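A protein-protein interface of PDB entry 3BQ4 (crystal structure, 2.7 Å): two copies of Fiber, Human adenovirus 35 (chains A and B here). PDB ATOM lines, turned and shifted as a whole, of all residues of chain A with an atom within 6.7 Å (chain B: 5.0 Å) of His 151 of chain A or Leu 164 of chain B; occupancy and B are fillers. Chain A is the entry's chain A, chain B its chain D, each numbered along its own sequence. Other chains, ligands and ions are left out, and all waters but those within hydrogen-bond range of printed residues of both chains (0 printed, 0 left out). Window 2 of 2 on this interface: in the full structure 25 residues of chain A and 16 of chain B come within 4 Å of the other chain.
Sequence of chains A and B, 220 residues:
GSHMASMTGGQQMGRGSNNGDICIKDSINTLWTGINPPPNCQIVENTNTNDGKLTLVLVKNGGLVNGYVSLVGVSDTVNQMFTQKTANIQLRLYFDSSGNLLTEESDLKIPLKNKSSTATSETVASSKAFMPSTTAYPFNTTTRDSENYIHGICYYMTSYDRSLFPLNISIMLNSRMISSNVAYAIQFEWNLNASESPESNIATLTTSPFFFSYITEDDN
N of Tyr 155 of chain B is in hydrogen-bond range of OG of Ser 208 of chain B, at 2.9 Å.
The backbone carbonyl oxygen (O) of Gly 152 of chain A lies within hydrogen-bond range of the backbone NH (N) of Ile 169 of chain A, 3.0 Å away.
Among the printed residues, pairs that only touch across the chains: Ile 153 of chain A with Tyr 155 of chain B (3.0 Å), His 151 of chain A with Tyr 155 of chain B (3.5 Å), His 151 of chain A with Leu 164 of chain B (3.6 Å) and Gly 152 of chain A with Tyr 155 of chain B (3.9 Å).
His 151 of chain A touches two residues of chain B.
Printed residues of chain B within 4 Å of Ile 153 of chain A: Tyr 155 (3.0 Å).
Of the printed residues of chain A, Tyr 155 of chain B touches His 151 (3.5 Å), Gly 152 (3.9 Å) and Ile 153 (3.0 Å).
Leu 164 of chain B touches just one residue of chain A: His 151 (3.6 Å).
The nearest printed residue of chain B that does not touch Gly 152 of chain A is Ser 208 of chain B (6.4 Å).
Hydrophobic or aromatic side chains of chain B within 4 Å of the printed part of chain A: Tyr 155 and Leu 164.
Printed residues of chain A that touch a printed residue of chain B: His 151, Gly 152 and Ile 153.
Hydrophobic or aromatic side chains of chain A within 4 Å of the printed part of chain B: His 151 and Ile 153.
Along chain A the printed residues that touch a printed residue of chain B span positions 151 to 153.
Among the printed residues, no Asp or Glu carboxylate lies within 4 Å of a Lys or Arg side-chain nitrogen of the other chain.
No position is printed for both chains.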
ATOM      1  N   ASN A 148     -18.469  15.584 -14.612  1.00  0.00           N
ATOM      2  CA  ASN A 148     -18.875  16.308 -13.426  1.00  0.00           C
ATOM      3  C   ASN A 148     -19.493  17.619 -13.894  1.00  0.00           C
ATOM      4  O   ASN A 148     -19.021  18.697 -13.576  1.00  0.00           O
ATOM      5  CB  ASN A 148     -17.694  16.554 -12.470  1.00  0.00           C
ATOM      6  CG  ASN A 148     -16.639  17.450 -13.055  1.00  0.00           C
ATOM      7  OD1 ASN A 148     -15.739  17.908 -12.346  1.00  0.00           O
ATOM      8  ND2 ASN A 148     -16.731  17.701 -14.354  1.00  0.00           N
ATOM      9  N   TYR A 149     -20.560  17.480 -14.671  1.00  0.00           N
ATOM     10  CA  TYR A 149     -21.321  18.592 -15.216  1.00  0.00           C
ATOM     11  C   TYR A 149     -22.814  18.348 -14.945  1.00  0.00           C
ATOM     12  O   TYR A 149     -23.280  17.204 -14.960  1.00  0.00           O
ATOM     13  CB  TYR A 149     -21.141  18.665 -16.734  1.00  0.00           C
ATOM     14  CG  TYR A 149     -19.916  19.379 -17.248  1.00  0.00           C
ATOM     15  CD1 TYR A 149     -18.700  18.711 -17.409  1.00  0.00           C
ATOM     16  CD2 TYR A 149     -19.989  20.714 -17.632  1.00  0.00           C
ATOM     17  CE1 TYR A 149     -17.584  19.358 -17.952  1.00  0.00           C
ATOM     18  CE2 TYR A 149     -18.888  21.371 -18.170  1.00  0.00           C
ATOM     19  CZ  TYR A 149     -17.688  20.693 -18.334  1.00  0.00           C
ATOM     20  OH  TYR A 149     -16.616  21.369 -18.890  1.00  0.00           O
ATOM     21  N   ILE A 150     -23.569  19.407 -14.703  1.00  0.00           N
ATOM     22  CA  ILE A 150     -24.996  19.236 -14.490  1.00  0.00           C
ATOM     23  C   ILE A 150     -25.716  19.956 -15.629  1.00  0.00           C
ATOM     24  O   ILE A 150     -25.723  21.180 -15.699  1.00  0.00           O
ATOM     25  CB  ILE A 150     -25.436  19.778 -13.103  1.00  0.00           C
ATOM     26  CG1 ILE A 150     -25.047  18.766 -12.015  1.00  0.00           C
ATOM     27  CG2 ILE A 150     -26.937  20.030 -13.086  1.00  0.00           C
ATOM     28  CD1 ILE A 150     -25.097  19.312 -10.611  1.00  0.00           C
ATOM     29  N   HIS A 151     -26.297  19.175 -16.533  1.00  0.00           N
ATOM     30  CA  HIS A 151     -27.006  19.705 -17.689  1.00  0.00           C
ATOM     31  C   HIS A 151     -28.518  19.652 -17.503  1.00  0.00           C
ATOM     32  O   HIS A 151     -29.070  18.678 -16.989  1.00  0.00           O
ATOM     33  CB  HIS A 151     -26.619  18.920 -18.951  1.00  0.00           C
ATOM     34  CG  HIS A 151     -25.147  18.688 -19.087  1.00  0.00           C
ATOM     35  ND1 HIS A 151     -24.253  19.695 -19.390  1.00  0.00           N
ATOM     36  CD2 HIS A 151     -24.406  17.567 -18.921  1.00  0.00           C
ATOM     37  CE1 HIS A 151     -23.027  19.203 -19.402  1.00  0.00           C
ATOM     38  NE2 HIS A 151     -23.091  17.913 -19.121  1.00  0.00           N
ATOM     39  N   GLY A 152     -29.173  20.714 -17.948  1.00  0.00           N
ATOM     40  CA  GLY A 152     -30.609  20.815 -17.833  1.00  0.00           C
ATOM     41  C   GLY A 152     -31.117  21.955 -18.699  1.00  0.00           C
ATOM     42  O   GLY A 152     -30.353  22.565 -19.447  1.00  0.00           O
ATOM     43  N   ILE A 153     -32.398  22.275 -18.557  1.00  0.00           N
ATOM     44  CA  ILE A 153     -33.035  23.291 -19.362  1.00  0.00           C
ATOM     45  C   ILE A 153     -33.841  24.302 -18.565  1.00  0.00           C
ATOM     46  O   ILE A 153     -34.698  23.920 -17.792  1.00  0.00           O
ATOM     47  CB  ILE A 153     -34.015  22.674 -20.376  1.00  0.00           C
ATOM     48  CG1 ILE A 153     -33.278  21.720 -21.316  1.00  0.00           C
ATOM     49  CG2 ILE A 153     -34.726  23.766 -21.161  1.00  0.00           C
ATOM     50  CD1 ILE A 153     -34.197  20.890 -22.187  1.00  0.00           C
ATOM     51  N   ASN A 168     -30.615  26.026 -22.775  1.00  0.00           N
ATOM     52  CA  ASN A 168     -29.707  25.107 -22.074  1.00  0.00           C
ATOM     53  C   ASN A 168     -28.865  25.741 -20.978  1.00  0.00           C
ATOM     54  O   ASN A 168     -28.269  26.792 -21.166  1.00  0.00           O
ATOM     55  CB  ASN A 168     -28.728  24.452 -23.058  1.00  0.00           C
ATOM     56  CG  ASN A 168     -29.404  23.525 -24.049  1.00  0.00           C
ATOM     57  OD1 ASN A 168     -29.969  22.500 -23.672  1.00  0.00           O
ATOM     58  ND2 ASN A 168     -29.343  23.883 -25.335  1.00  0.00           N
ATOM     59  N   ILE A 169     -28.797  25.068 -19.841  1.00  0.00           N
ATOM     60  CA  ILE A 169     -28.010  25.536 -18.710  1.00  0.00           C
ATOM     61  C   ILE A 169     -27.098  24.386 -18.343  1.00  0.00           C
ATOM     62  O   ILE A 169     -27.449  23.216 -18.548  1.00  0.00           O
ATOM     63  CB  ILE A 169     -28.918  25.891 -17.469  1.00  0.00           C
ATOM     64  CG1 ILE A 169     -28.077  26.009 -16.194  1.00  0.00           C
ATOM     65  CG2 ILE A 169     -30.002  24.837 -17.295  1.00  0.00           C
ATOM     66  CD1 ILE A 169     -28.238  27.317 -15.483  1.00  0.00           C
ATOM     67  N   SER A 170     -25.904  24.696 -17.861  1.00  0.00           N
ATOM     68  CA  SER A 170     -25.021  23.630 -17.437  1.00  0.00           C
ATOM     69  C   SER A 170     -24.069  24.165 -16.386  1.00  0.00           C
ATOM     70  O   SER A 170     -23.476  25.233 -16.546  1.00  0.00           O
ATOM     71  CB  SER A 170     -24.299  22.982 -18.631  1.00  0.00           C
ATOM     72  OG  SER A 170     -23.629  23.912 -19.427  1.00  0.00           O
ATOM     73  N   ILE A 171     -23.980  23.424 -15.286  1.00  0.00           N
ATOM     74  CA  ILE A 171     -23.155  23.788 -14.157  1.00  0.00           C
ATOM     75  C   ILE A 171     -21.938  22.910 -14.034  1.00  0.00           C
ATOM     76  O   ILE A 171     -22.057  21.699 -13.731  1.00  0.00           O
ATOM     77  CB  ILE A 171     -23.942  23.656 -12.884  1.00  0.00           C
ATOM     78  CG1 ILE A 171     -25.305  24.333 -13.106  1.00  0.00           C
ATOM     79  CG2 ILE A 171     -23.087  24.190 -11.710  1.00  0.00           C
ATOM     80  CD1 ILE A 171     -26.283  24.213 -12.010  1.00  0.00           C
ATOM     81  N   PHE A 210     -33.512  27.592 -12.010  1.00  0.00           N
ATOM     82  CA  PHE A 210     -33.111  26.227 -12.315  1.00  0.00           C
ATOM     83  C   PHE A 210     -32.656  25.582 -11.027  1.00  0.00           C
ATOM     84  O   PHE A 210     -31.845  26.165 -10.307  1.00  0.00           O
ATOM     85  CB  PHE A 210     -31.970  26.222 -13.325  1.00  0.00           C
ATOM     86  CG  PHE A 210     -31.394  24.863 -13.579  1.00  0.00           C
ATOM     87  CD1 PHE A 210     -32.085  23.924 -14.302  1.00  0.00           C
ATOM     88  CD2 PHE A 210     -30.152  24.517 -13.080  1.00  0.00           C
ATOM     89  CE1 PHE A 210     -31.537  22.645 -14.529  1.00  0.00           C
ATOM     90  CE2 PHE A 210     -29.612  23.244 -13.304  1.00  0.00           C
ATOM     91  CZ  PHE A 210     -30.313  22.319 -14.027  1.00  0.00           C
ATOM     92  N   TYR B 155     -28.773  13.836 -19.393  1.00  0.00           N
ATOM     93  CA  TYR B 155     -28.005  13.949 -20.612  1.00  0.00           C
ATOM     94  C   TYR B 155     -26.703  13.178 -20.646  1.00  0.00           C
ATOM     95  O   TYR B 155     -26.093  12.961 -19.607  1.00  0.00           O
ATOM     96  CB  TYR B 155     -27.703  15.430 -20.861  1.00  0.00           C
ATOM     97  CG  TYR B 155     -28.933  16.297 -21.030  1.00  0.00           C
ATOM     98  CD1 TYR B 155     -29.574  16.873 -19.924  1.00  0.00           C
ATOM     99  CD2 TYR B 155     -29.481  16.521 -22.302  1.00  0.00           C
ATOM    100  CE1 TYR B 155     -30.746  17.626 -20.087  1.00  0.00           C
ATOM    101  CE2 TYR B 155     -30.619  17.283 -22.478  1.00  0.00           C
ATOM    102  CZ  TYR B 155     -31.256  17.828 -21.371  1.00  0.00           C
ATOM    103  OH  TYR B 155     -32.444  18.515 -21.560  1.00  0.00           O
ATOM    104  N   TYR B 156     -26.300  12.757 -21.848  1.00  0.00           N
ATOM    105  CA  TYR B 156     -25.029  12.068 -22.059  1.00  0.00           C
ATOM    106  C   TYR B 156     -24.072  12.931 -22.893  1.00  0.00           C
ATOM    107  O   TYR B 156     -24.415  13.354 -23.995  1.00  0.00           O
ATOM    108  CB  TYR B 156     -25.209  10.751 -22.786  1.00  0.00           C
ATOM    109  CG  TYR B 156     -23.874  10.109 -23.094  1.00  0.00           C
ATOM    110  CD1 TYR B 156     -23.034   9.664 -22.067  1.00  0.00           C
ATOM    111  CD2 TYR B 156     -23.438   9.971 -24.412  1.00  0.00           C
ATOM    112  CE1 TYR B 156     -21.793   9.092 -22.355  1.00  0.00           C
ATOM    113  CE2 TYR B 156     -22.203   9.406 -24.709  1.00  0.00           C
ATOM    114  CZ  TYR B 156     -21.386   8.969 -23.685  1.00  0.00           C
ATOM    115  OH  TYR B 156     -20.166   8.414 -24.002  1.00  0.00           O
ATOM    116  N   MET B 157     -22.875  13.183 -22.368  1.00  0.00           N
ATOM    117  CA  MET B 157     -21.877  13.984 -23.077  1.00  0.00           C
ATOM    118  C   MET B 157     -21.033  13.044 -23.930  1.00  0.00           C
ATOM    119  O   MET B 157     -20.439  12.090 -23.429  1.00  0.00           O
ATOM    120  CB  MET B 157     -20.984  14.745 -22.088  1.00  0.00           C
ATOM    121  CG  MET B 157     -20.249  15.951 -22.671  1.00  0.00           C
ATOM    122  SD  MET B 157     -19.439  16.970 -21.385  1.00  0.00           S
ATOM    123  CE  MET B 157     -18.227  15.778 -20.758  1.00  0.00           C
ATOM    124  N   THR B 158     -21.013  13.326 -25.230  1.00  0.00           N
ATOM    125  CA  THR B 158     -20.275  12.556 -26.224  1.00  0.00           C
ATOM    126  C   THR B 158     -18.783  12.394 -25.923  1.00  0.00           C
ATOM    127  O   THR B 158     -18.144  13.303 -25.407  1.00  0.00           O
ATOM    128  CB  THR B 158     -20.431  13.215 -27.580  1.00  0.00           C
ATOM    129  OG1 THR B 158     -20.485  14.633 -27.399  1.00  0.00           O
ATOM    130  CG2 THR B 158     -21.708  12.763 -28.246  1.00  0.00           C
ATOM    131  N   ARG B 162     -18.011  16.941 -27.537  1.00  0.00           N
ATOM    132  CA  ARG B 162     -18.563  17.139 -26.205  1.00  0.00           C
ATOM    133  C   ARG B 162     -20.074  17.373 -26.251  1.00  0.00           C
ATOM    134  O   ARG B 162     -20.641  17.974 -25.341  1.00  0.00           O
ATOM    135  CB  ARG B 162     -17.876  18.330 -25.548  1.00  0.00           C
ATOM    136  CG  ARG B 162     -18.097  18.423 -24.059  1.00  0.00           C
ATOM    137  CD  ARG B 162     -16.935  17.815 -23.298  1.00  0.00           C
ATOM    138  NE  ARG B 162     -16.622  16.459 -23.738  1.00  0.00           N
ATOM    139  CZ  ARG B 162     -15.609  15.742 -23.261  1.00  0.00           C
ATOM    140  NH1 ARG B 162     -14.813  16.254 -22.331  1.00  0.00           N
ATOM    141  NH2 ARG B 162     -15.386  14.514 -23.717  1.00  0.00           N
ATOM    142  N   SER B 163     -20.727  16.897 -27.307  1.00  0.00           N
ATOM    143  CA  SER B 163     -22.169  17.086 -27.458  1.00  0.00           C
ATOM    144  C   SER B 163     -23.003  16.449 -26.352  1.00  0.00           C
ATOM    145  O   SER B 163     -22.514  15.627 -25.580  1.00  0.00           O
ATOM    146  CB  SER B 163     -22.639  16.555 -28.811  1.00  0.00           C
ATOM    147  OG  SER B 163     -24.029  16.768 -28.977  1.00  0.00           O
ATOM    148  N   LEU B 164     -24.276  16.830 -26.295  1.00  0.00           N
ATOM    149  CA  LEU B 164     -25.191  16.327 -25.273  1.00  0.00           C
ATOM    150  C   LEU B 164     -26.434  15.660 -25.866  1.00  0.00           C
ATOM    151  O   LEU B 164     -27.248  16.308 -26.528  1.00  0.00           O
ATOM    152  CB  LEU B 164     -25.629  17.483 -24.345  1.00  0.00           C
ATOM    153  CG  LEU B 164     -24.549  18.241 -23.566  1.00  0.00           C
ATOM    154  CD1 LEU B 164     -25.181  19.425 -22.858  1.00  0.00           C
ATOM    155  CD2 LEU B 164     -23.854  17.297 -22.576  1.00  0.00           C
ATOM    156  N   PHE B 165     -26.589  14.363 -25.626  1.00  0.00           N
ATOM    157  CA  PHE B 165     -27.766  13.654 -26.120  1.00  0.00           C
ATOM    158  C   PHE B 165     -28.754  13.401 -24.988  1.00  0.00           C
ATOM    159  O   PHE B 165     -28.404  12.821 -23.961  1.00  0.00           O
ATOM    160  CB  PHE B 165     -27.366  12.330 -26.773  1.00  0.00           C
ATOM    161  CG  PHE B 165     -26.540  12.500 -28.006  1.00  0.00           C
ATOM    162  CD1 PHE B 165     -25.428  11.689 -28.225  1.00  0.00           C
ATOM    163  CD2 PHE B 165     -26.829  13.519 -28.919  1.00  0.00           C
ATOM    164  CE1 PHE B 165     -24.603  11.888 -29.333  1.00  0.00           C
ATOM    165  CE2 PHE B 165     -26.016  13.729 -30.031  1.00  0.00           C
ATOM    166  CZ  PHE B 165     -24.894  12.911 -30.237  1.00  0.00           C
ATOM    167  N   PRO B 166     -30.001  13.859 -25.155  1.00  0.00           N
ATOM    168  CA  PRO B 166     -31.029  13.666 -24.132  1.00  0.00           C
ATOM    169  C   PRO B 166     -31.468  12.216 -24.005  1.00  0.00           C
ATOM    170  O   PRO B 166     -31.964  11.633 -24.961  1.00  0.00           O
ATOM    171  CB  PRO B 166     -32.169  14.563 -24.617  1.00  0.00           C
ATOM    172  CG  PRO B 166     -32.003  14.529 -26.098  1.00  0.00           C
ATOM    173  CD  PRO B 166     -30.513  14.694 -26.250  1.00  0.00           C
ATOM    174  N   SER B 208     -25.800  12.009 -16.767  1.00  0.00           N
ATOM    175  CA  SER B 208     -25.688  13.203 -15.933  1.00  0.00           C
ATOM    176  C   SER B 208     -26.669  13.133 -14.751  1.00  0.00           C
ATOM    177  O   SER B 208     -27.699  12.454 -14.814  1.00  0.00           O
ATOM    178  CB  SER B 208     -25.924  14.476 -16.766  1.00  0.00           C
ATOM    179  OG  SER B 208     -27.283  14.677 -17.098  1.00  0.00           O
